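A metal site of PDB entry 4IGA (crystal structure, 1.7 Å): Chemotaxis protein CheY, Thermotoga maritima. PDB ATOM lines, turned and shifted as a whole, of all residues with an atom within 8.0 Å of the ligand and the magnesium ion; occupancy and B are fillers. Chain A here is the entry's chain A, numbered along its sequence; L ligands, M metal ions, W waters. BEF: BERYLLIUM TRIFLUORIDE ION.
F2 of the ligand sits at hydrogen-bond distance from OG of Ser 85 (2.6 Å). F2 of the ligand lies within hydrogen-bond range of N of Ile 58 (3.0 Å). The side-chain amino group of Lys 107 is in hydrogen-bond range of a fluorine (F1) of the ligand (2.9 Å). The side-chain carboxylate (OD1) of Asp 57 is bound to a beryllium atom (BE) of the ligand (2.0 Å). F1 of the ligand lies within hydrogen-bond range of N of Ala 86, 2.7 Å away. The backbone NH (N) of Thr 59 sits at hydrogen-bond distance from a fluorine (F2) of the ligand, 2.8 Å away.
The backbone carbonyl oxygen of Ile 58 is in hydrogen-bond range of the backbone NH of Gly 65. N of Lys 107 is in hydrogen-bond range of O of Ser 85 (3.0 Å). OG of Ser 85 lies within hydrogen-bond range of N of Met 87 (2.9 Å). The backbone carbonyl oxygen of Ile 105 is in hydrogen-bond range of the backbone NH of Ser 85. The side-chain carboxylate (OD1) of Asp 57 sits close to the side-chain amino group (NZ) of Lys 107, 3.5 Å away. N of Asp 57 sits at hydrogen-bond distance from O of Val 11. The side-chain carboxylate (OD2) of Asp 12 lies within salt-bridge range of the side-chain amino group (NZ) of Lys 107 (2.9 Å).
Of the 25 residues printed, 6 come within 4 Å of the ligand. Along chain A the residues within 4 Å of the ligand span positions 57 to 107.
The nearest printed residue that does not touch the magnesium ion is Asp 12 (4.1 Å).
The magnesium ion is bound by water W1 (1.9 Å), water W2 (2.0 Å), F3 of the ligand (2.0 Å), OD2 of Asp 57 (2.0 Å), O of Thr 59 (2.1 Å) and OD1 of Asp 13 (2.3 Å). The magnesium ion has six donor atoms within binding distance.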
ATOM      1  N   VAL A  11       3.272  -4.895   0.969  1.00  0.00           N
ATOM      2  CA  VAL A  11       2.516  -5.024  -0.279  1.00  0.00           C
ATOM      3  C   VAL A  11       2.225  -3.690  -0.926  1.00  0.00           C
ATOM      4  O   VAL A  11       1.469  -2.889  -0.385  1.00  0.00           O
ATOM      5  CB  VAL A  11       1.135  -5.705  -0.010  1.00  0.00           C
ATOM      6  CG1 VAL A  11       0.397  -6.067  -1.383  1.00  0.00           C
ATOM      7  CG2 VAL A  11       1.324  -6.948   0.816  1.00  0.00           C
ATOM      8  N   ASP A  12       2.741  -3.477  -2.146  1.00  0.00           N
ATOM      9  CA  ASP A  12       2.457  -2.211  -2.869  1.00  0.00           C
ATOM     10  C   ASP A  12       2.924  -2.404  -4.288  1.00  0.00           C
ATOM     11  O   ASP A  12       4.027  -2.969  -4.543  1.00  0.00           O
ATOM     12  CB  ASP A  12       3.239  -1.049  -2.190  1.00  0.00           C
ATOM     13  CG  ASP A  12       2.744   0.339  -2.624  1.00  0.00           C
ATOM     14  OD1 ASP A  12       2.799   0.653  -3.816  1.00  0.00           O
ATOM     15  OD2 ASP A  12       2.346   1.126  -1.749  1.00  0.00           O
ATOM     16  N   ASP A  13       2.128  -1.902  -5.276  1.00  0.00           N
ATOM     17  CA  ASP A  13       2.618  -2.045  -6.643  1.00  0.00           C
ATOM     18  C   ASP A  13       3.727  -1.072  -7.062  1.00  0.00           C
ATOM     19  O   ASP A  13       4.316  -1.269  -8.111  1.00  0.00           O
ATOM     20  CB  ASP A  13       1.453  -2.006  -7.591  1.00  0.00           C
ATOM     21  CG  ASP A  13       0.682  -0.732  -7.510  1.00  0.00           C
ATOM     22  OD1 ASP A  13       0.449  -0.189  -6.415  1.00  0.00           O
ATOM     23  OD2 ASP A  13       0.279  -0.308  -8.581  1.00  0.00           O
ATOM     24  N   ALA A  14       4.047  -0.082  -6.206  1.00  0.00           N
ATOM     25  CA  ALA A  14       5.071   0.953  -6.564  1.00  0.00           C
ATOM     26  C   ALA A  14       6.399   0.517  -6.019  1.00  0.00           C
ATOM     27  O   ALA A  14       6.572   0.492  -4.812  1.00  0.00           O
ATOM     28  CB  ALA A  14       4.752   2.282  -5.941  1.00  0.00           C
ATOM     29  N   MET A  17       7.832   3.023  -3.258  1.00  0.00           N
ATOM     30  CA  MET A  17       7.194   2.836  -1.961  1.00  0.00           C
ATOM     31  C   MET A  17       7.686   1.567  -1.239  1.00  0.00           C
ATOM     32  O   MET A  17       8.026   1.612  -0.055  1.00  0.00           O
ATOM     33  CB  MET A  17       5.676   2.761  -2.133  1.00  0.00           C
ATOM     34  CG  MET A  17       4.928   2.744  -0.765  1.00  0.00           C
ATOM     35  SD  MET A  17       5.366   4.209   0.227  1.00  0.00           S
ATOM     36  CE  MET A  17       4.833   5.594  -0.806  1.00  0.00           C
ATOM     37  N   THR A  37       3.443  -7.356  -5.038  1.00  0.00           N
ATOM     38  CA  THR A  37       3.201  -6.195  -5.879  1.00  0.00           C
ATOM     39  C   THR A  37       1.736  -6.050  -6.310  1.00  0.00           C
ATOM     40  O   THR A  37       1.391  -5.156  -7.083  1.00  0.00           O
ATOM     41  CB  THR A  37       4.114  -6.201  -7.163  1.00  0.00           C
ATOM     42  OG1 THR A  37       3.679  -7.224  -8.030  1.00  0.00           O
ATOM     43  CG2 THR A  37       5.595  -6.495  -6.822  1.00  0.00           C
ATOM     44  N   MET A  56      -0.145  -2.828   3.669  1.00  0.00           N
ATOM     45  CA  MET A  56      -1.045  -3.055   2.523  1.00  0.00           C
ATOM     46  C   MET A  56      -1.425  -1.785   1.811  1.00  0.00           C
ATOM     47  O   MET A  56      -2.179  -0.971   2.383  1.00  0.00           O
ATOM     48  CB  MET A  56      -2.315  -3.788   2.989  1.00  0.00           C
ATOM     49  CG  MET A  56      -3.299  -4.113   1.842  1.00  0.00           C
ATOM     50  SD  MET A  56      -2.717  -5.440   0.729  1.00  0.00           S
ATOM     51  CE  MET A  56      -2.627  -6.905   1.785  1.00  0.00           C
ATOM     52  N   ASP A  57      -1.021  -1.690   0.536  1.00  0.00           N
ATOM     53  CA  ASP A  57      -1.534  -0.649  -0.390  1.00  0.00           C
ATOM     54  C   ASP A  57      -2.974  -1.007  -0.795  1.00  0.00           C
ATOM     55  O   ASP A  57      -3.359  -2.180  -0.664  1.00  0.00           O
ATOM     56  CB  ASP A  57      -0.680  -0.693  -1.643  1.00  0.00           C
ATOM     57  CG  ASP A  57      -0.957   0.481  -2.593  1.00  0.00           C
ATOM     58  OD1 ASP A  57      -1.469   1.533  -2.143  1.00  0.00           O
ATOM     59  OD2 ASP A  57      -0.665   0.348  -3.794  1.00  0.00           O
ATOM     60  N   ILE A  58      -3.768  -0.037  -1.281  1.00  0.00           N
ATOM     61  CA  ILE A  58      -5.133  -0.325  -1.840  1.00  0.00           C
ATOM     62  C   ILE A  58      -5.148  -0.486  -3.373  1.00  0.00           C
ATOM     63  O   ILE A  58      -5.544  -1.550  -3.893  1.00  0.00           O
ATOM     64  CB  ILE A  58      -6.258   0.708  -1.353  1.00  0.00           C
ATOM     65  CG1 ILE A  58      -6.490   0.591   0.201  1.00  0.00           C
ATOM     66  CG2 ILE A  58      -7.584   0.432  -2.088  1.00  0.00           C
ATOM     67  CD1 ILE A  58      -6.772  -0.779   0.732  1.00  0.00           C
ATOM     68  N   THR A  59      -4.669   0.516  -4.067  1.00  0.00           N
ATOM     69  CA  THR A  59      -4.815   0.610  -5.569  1.00  0.00           C
ATOM     70  C   THR A  59      -3.703  -0.203  -6.174  1.00  0.00           C
ATOM     71  O   THR A  59      -2.526   0.212  -6.159  1.00  0.00           O
ATOM     72  CB  THR A  59      -4.780   2.054  -6.018  1.00  0.00           C
ATOM     73  OG1 THR A  59      -5.813   2.785  -5.352  1.00  0.00           O
ATOM     74  CG2 THR A  59      -4.925   2.203  -7.585  1.00  0.00           C
ATOM     75  N   MET A  60      -4.061  -1.356  -6.743  1.00  0.00           N
ATOM     76  CA  MET A  60      -3.041  -2.245  -7.330  1.00  0.00           C
ATOM     77  C   MET A  60      -3.664  -2.921  -8.468  1.00  0.00           C
ATOM     78  O   MET A  60      -4.891  -3.126  -8.444  1.00  0.00           O
ATOM     79  CB  MET A  60      -2.578  -3.341  -6.349  1.00  0.00           C
ATOM     80  CG  MET A  60      -1.873  -2.776  -5.138  1.00  0.00           C
ATOM     81  SD  MET A  60      -1.229  -3.981  -3.942  1.00  0.00           S
ATOM     82  CE  MET A  60      -2.676  -4.652  -3.136  1.00  0.00           C
ATOM     83  N   PRO A  61      -2.840  -3.321  -9.439  1.00  0.00           N
ATOM     84  CA  PRO A  61      -3.357  -4.087 -10.551  1.00  0.00           C
ATOM     85  C   PRO A  61      -3.789  -5.466 -10.039  1.00  0.00           C
ATOM     86  O   PRO A  61      -3.331  -5.911  -8.965  1.00  0.00           O
ATOM     87  CB  PRO A  61      -2.151  -4.199 -11.497  1.00  0.00           C
ATOM     88  CG  PRO A  61      -1.241  -3.062 -11.098  1.00  0.00           C
ATOM     89  CD  PRO A  61      -1.414  -3.001  -9.615  1.00  0.00           C
ATOM     90  N   ASN A  64      -7.197  -5.501  -5.749  1.00  0.00           N
ATOM     91  CA  ASN A  64      -6.886  -4.415  -4.839  1.00  0.00           C
ATOM     92  C   ASN A  64      -6.629  -4.860  -3.386  1.00  0.00           C
ATOM     93  O   ASN A  64      -6.760  -6.065  -3.021  1.00  0.00           O
ATOM     94  CB  ASN A  64      -7.882  -3.251  -4.937  1.00  0.00           C
ATOM     95  CG  ASN A  64      -9.237  -3.546  -4.320  1.00  0.00           C
ATOM     96  OD1 ASN A  64      -9.363  -4.418  -3.485  1.00  0.00           O
ATOM     97  ND2 ASN A  64     -10.270  -2.820  -4.755  1.00  0.00           N
ATOM     98  N   GLY A  65      -6.225  -3.889  -2.573  1.00  0.00           N
ATOM     99  CA  GLY A  65      -5.936  -4.116  -1.148  1.00  0.00           C
ATOM    100  C   GLY A  65      -7.119  -4.615  -0.333  1.00  0.00           C
ATOM    101  O   GLY A  65      -6.914  -5.351   0.639  1.00  0.00           O
ATOM    102  N   VAL A  83      -2.932  -0.748   6.652  1.00  0.00           N
ATOM    103  CA  VAL A  83      -3.084  -0.169   5.333  1.00  0.00           C
ATOM    104  C   VAL A  83      -2.178   1.045   5.257  1.00  0.00           C
ATOM    105  O   VAL A  83      -2.005   1.785   6.234  1.00  0.00           O
ATOM    106  CB  VAL A  83      -4.564   0.209   5.007  1.00  0.00           C
ATOM    107  CG1 VAL A  83      -4.751   1.011   3.627  1.00  0.00           C
ATOM    108  CG2 VAL A  83      -5.360  -1.042   4.912  1.00  0.00           C
ATOM    109  N   CYS A  84      -1.594   1.211   4.053  1.00  0.00           N
ATOM    110  CA  CYS A  84      -0.734   2.352   3.739  1.00  0.00           C
ATOM    111  C   CYS A  84      -1.084   2.739   2.292  1.00  0.00           C
ATOM    112  O   CYS A  84      -0.665   2.062   1.353  1.00  0.00           O
ATOM    113  CB  CYS A  84       0.765   2.033   4.003  1.00  0.00           C
ATOM    114  SG  CYS A  84       1.745   3.470   3.663  1.00  0.00           S
ATOM    115  N   SER A  85      -1.947   3.768   2.126  1.00  0.00           N
ATOM    116  CA  SER A  85      -2.589   4.062   0.802  1.00  0.00           C
ATOM    117  C   SER A  85      -2.894   5.538   0.593  1.00  0.00           C
ATOM    118  O   SER A  85      -3.133   6.263   1.573  1.00  0.00           O
ATOM    119  CB  SER A  85      -3.890   3.231   0.738  1.00  0.00           C
ATOM    120  OG  SER A  85      -4.701   3.532  -0.404  1.00  0.00           O
ATOM    121  N   ALA A  86      -2.870   5.963  -0.663  1.00  0.00           N
ATOM    122  CA  ALA A  86      -3.310   7.298  -1.114  1.00  0.00           C
ATOM    123  C   ALA A  86      -4.821   7.428  -0.982  1.00  0.00           C
ATOM    124  O   ALA A  86      -5.313   8.527  -0.929  1.00  0.00           O
ATOM    125  CB  ALA A  86      -2.905   7.531  -2.551  1.00  0.00           C
ATOM    126  N   MET A  87      -5.537   6.301  -0.906  1.00  0.00           N
ATOM    127  CA  MET A  87      -7.021   6.284  -0.871  1.00  0.00           C
ATOM    128  C   MET A  87      -7.524   6.473   0.572  1.00  0.00           C
ATOM    129  O   MET A  87      -8.068   5.530   1.158  1.00  0.00           O
ATOM    130  CB  MET A  87      -7.593   4.976  -1.461  1.00  0.00           C
ATOM    131  CG  MET A  87      -7.317   4.752  -2.934  1.00  0.00           C
ATOM    132  SD  MET A  87      -8.284   5.849  -3.991  1.00  0.00           S
ATOM    133  CE  MET A  87      -7.348   5.784  -5.512  1.00  0.00           C
ATOM    134  N   GLY A  88      -7.328   7.695   1.105  1.00  0.00           N
ATOM    135  CA  GLY A  88      -7.664   8.032   2.489  1.00  0.00           C
ATOM    136  C   GLY A  88      -9.040   8.628   2.731  1.00  0.00           C
ATOM    137  O   GLY A  88      -9.241   9.300   3.732  1.00  0.00           O
ATOM    138  N   MET A  92     -13.191   4.554   2.190  1.00  0.00           N
ATOM    139  CA  MET A  92     -12.155   3.534   2.012  1.00  0.00           C
ATOM    140  C   MET A  92     -11.608   3.063   3.379  1.00  0.00           C
ATOM    141  O   MET A  92     -11.322   1.838   3.580  1.00  0.00           O
ATOM    142  CB  MET A  92     -11.009   4.028   1.119  1.00  0.00           C
ATOM    143  CG  MET A  92     -10.018   2.904   0.795  1.00  0.00           C
ATOM    144  SD  MET A  92     -10.639   1.601  -0.283  1.00  0.00           S
ATOM    145  CE  MET A  92     -10.546   2.402  -1.896  1.00  0.00           C
ATOM    146  N   PHE A 104      -4.645   2.281   9.678  1.00  0.00           N
ATOM    147  CA  PHE A 104      -4.696   2.887   8.336  1.00  0.00           C
ATOM    148  C   PHE A 104      -3.800   4.188   8.335  1.00  0.00           C
ATOM    149  O   PHE A 104      -3.964   5.086   9.166  1.00  0.00           O
ATOM    150  CB  PHE A 104      -6.170   3.231   7.963  1.00  0.00           C
ATOM    151  CG  PHE A 104      -6.407   3.545   6.491  1.00  0.00           C
ATOM    152  CD1 PHE A 104      -5.782   4.633   5.870  1.00  0.00           C
ATOM    153  CD2 PHE A 104      -7.263   2.761   5.734  1.00  0.00           C
ATOM    154  CE1 PHE A 104      -6.019   4.925   4.482  1.00  0.00           C
ATOM    155  CE2 PHE A 104      -7.507   3.055   4.384  1.00  0.00           C
ATOM    156  CZ  PHE A 104      -6.915   4.138   3.778  1.00  0.00           C
ATOM    157  N   ILE A 105      -2.851   4.255   7.410  1.00  0.00           N
ATOM    158  CA  ILE A 105      -1.927   5.370   7.232  1.00  0.00           C
ATOM    159  C   ILE A 105      -2.162   5.883   5.810  1.00  0.00           C
ATOM    160  O   ILE A 105      -2.010   5.141   4.813  1.00  0.00           O
ATOM    161  CB  ILE A 105      -0.454   4.895   7.409  1.00  0.00           C
ATOM    162  CG1 ILE A 105      -0.276   4.276   8.807  1.00  0.00           C
ATOM    163  CG2 ILE A 105       0.536   6.047   7.170  1.00  0.00           C
ATOM    164  CD1 ILE A 105       1.136   3.726   9.068  1.00  0.00           C
ATOM    165  N   VAL A 106      -2.539   7.153   5.721  1.00  0.00           N
ATOM    166  CA  VAL A 106      -2.714   7.823   4.423  1.00  0.00           C
ATOM    167  C   VAL A 106      -1.344   8.355   3.917  1.00  0.00           C
ATOM    168  O   VAL A 106      -0.532   8.809   4.717  1.00  0.00           O
ATOM    169  CB  VAL A 106      -3.821   8.913   4.512  1.00  0.00           C
ATOM    170  CG1 VAL A 106      -3.391  10.068   5.492  1.00  0.00           C
ATOM    171  CG2 VAL A 106      -4.197   9.475   3.131  1.00  0.00           C
ATOM    172  N   LYS A 107      -1.106   8.181   2.606  1.00  0.00           N
ATOM    173  CA  LYS A 107       0.005   8.774   1.853  1.00  0.00           C
ATOM    174  C   LYS A 107      -0.318  10.212   1.387  1.00  0.00           C
ATOM    175  O   LYS A 107      -1.465  10.520   1.079  1.00  0.00           O
ATOM    176  CB  LYS A 107       0.242   7.992   0.600  1.00  0.00           C
ATOM    177  CG  LYS A 107       0.728   6.554   0.852  1.00  0.00           C
ATOM    178  CD  LYS A 107       0.811   5.870  -0.466  1.00  0.00           C
ATOM    179  CE  LYS A 107       1.280   4.445  -0.249  1.00  0.00           C
ATOM    180  NZ  LYS A 107       1.213   3.757  -1.535  1.00  0.00           N
HETATM  181 BE   BEF L   1      -2.189   3.260  -2.978  1.00  0.00          BE
HETATM  182  F1  BEF L   1      -1.516   4.303  -2.363  1.00  0.00           F
HETATM  183  F2  BEF L   1      -3.638   2.618  -2.603  1.00  0.00           F
HETATM  184  F3  BEF L   1      -1.842   2.738  -4.389  1.00  0.00           F
HETATM  185 MG    MG M   1      -0.881   1.388  -5.511  1.00  0.00          MG
HETATM  186  O   HOH W   1      -0.894   2.638  -6.926  1.00  0.00           O
HETATM  187  O   HOH W   2       0.843   2.165  -4.914  1.00  0.00           O
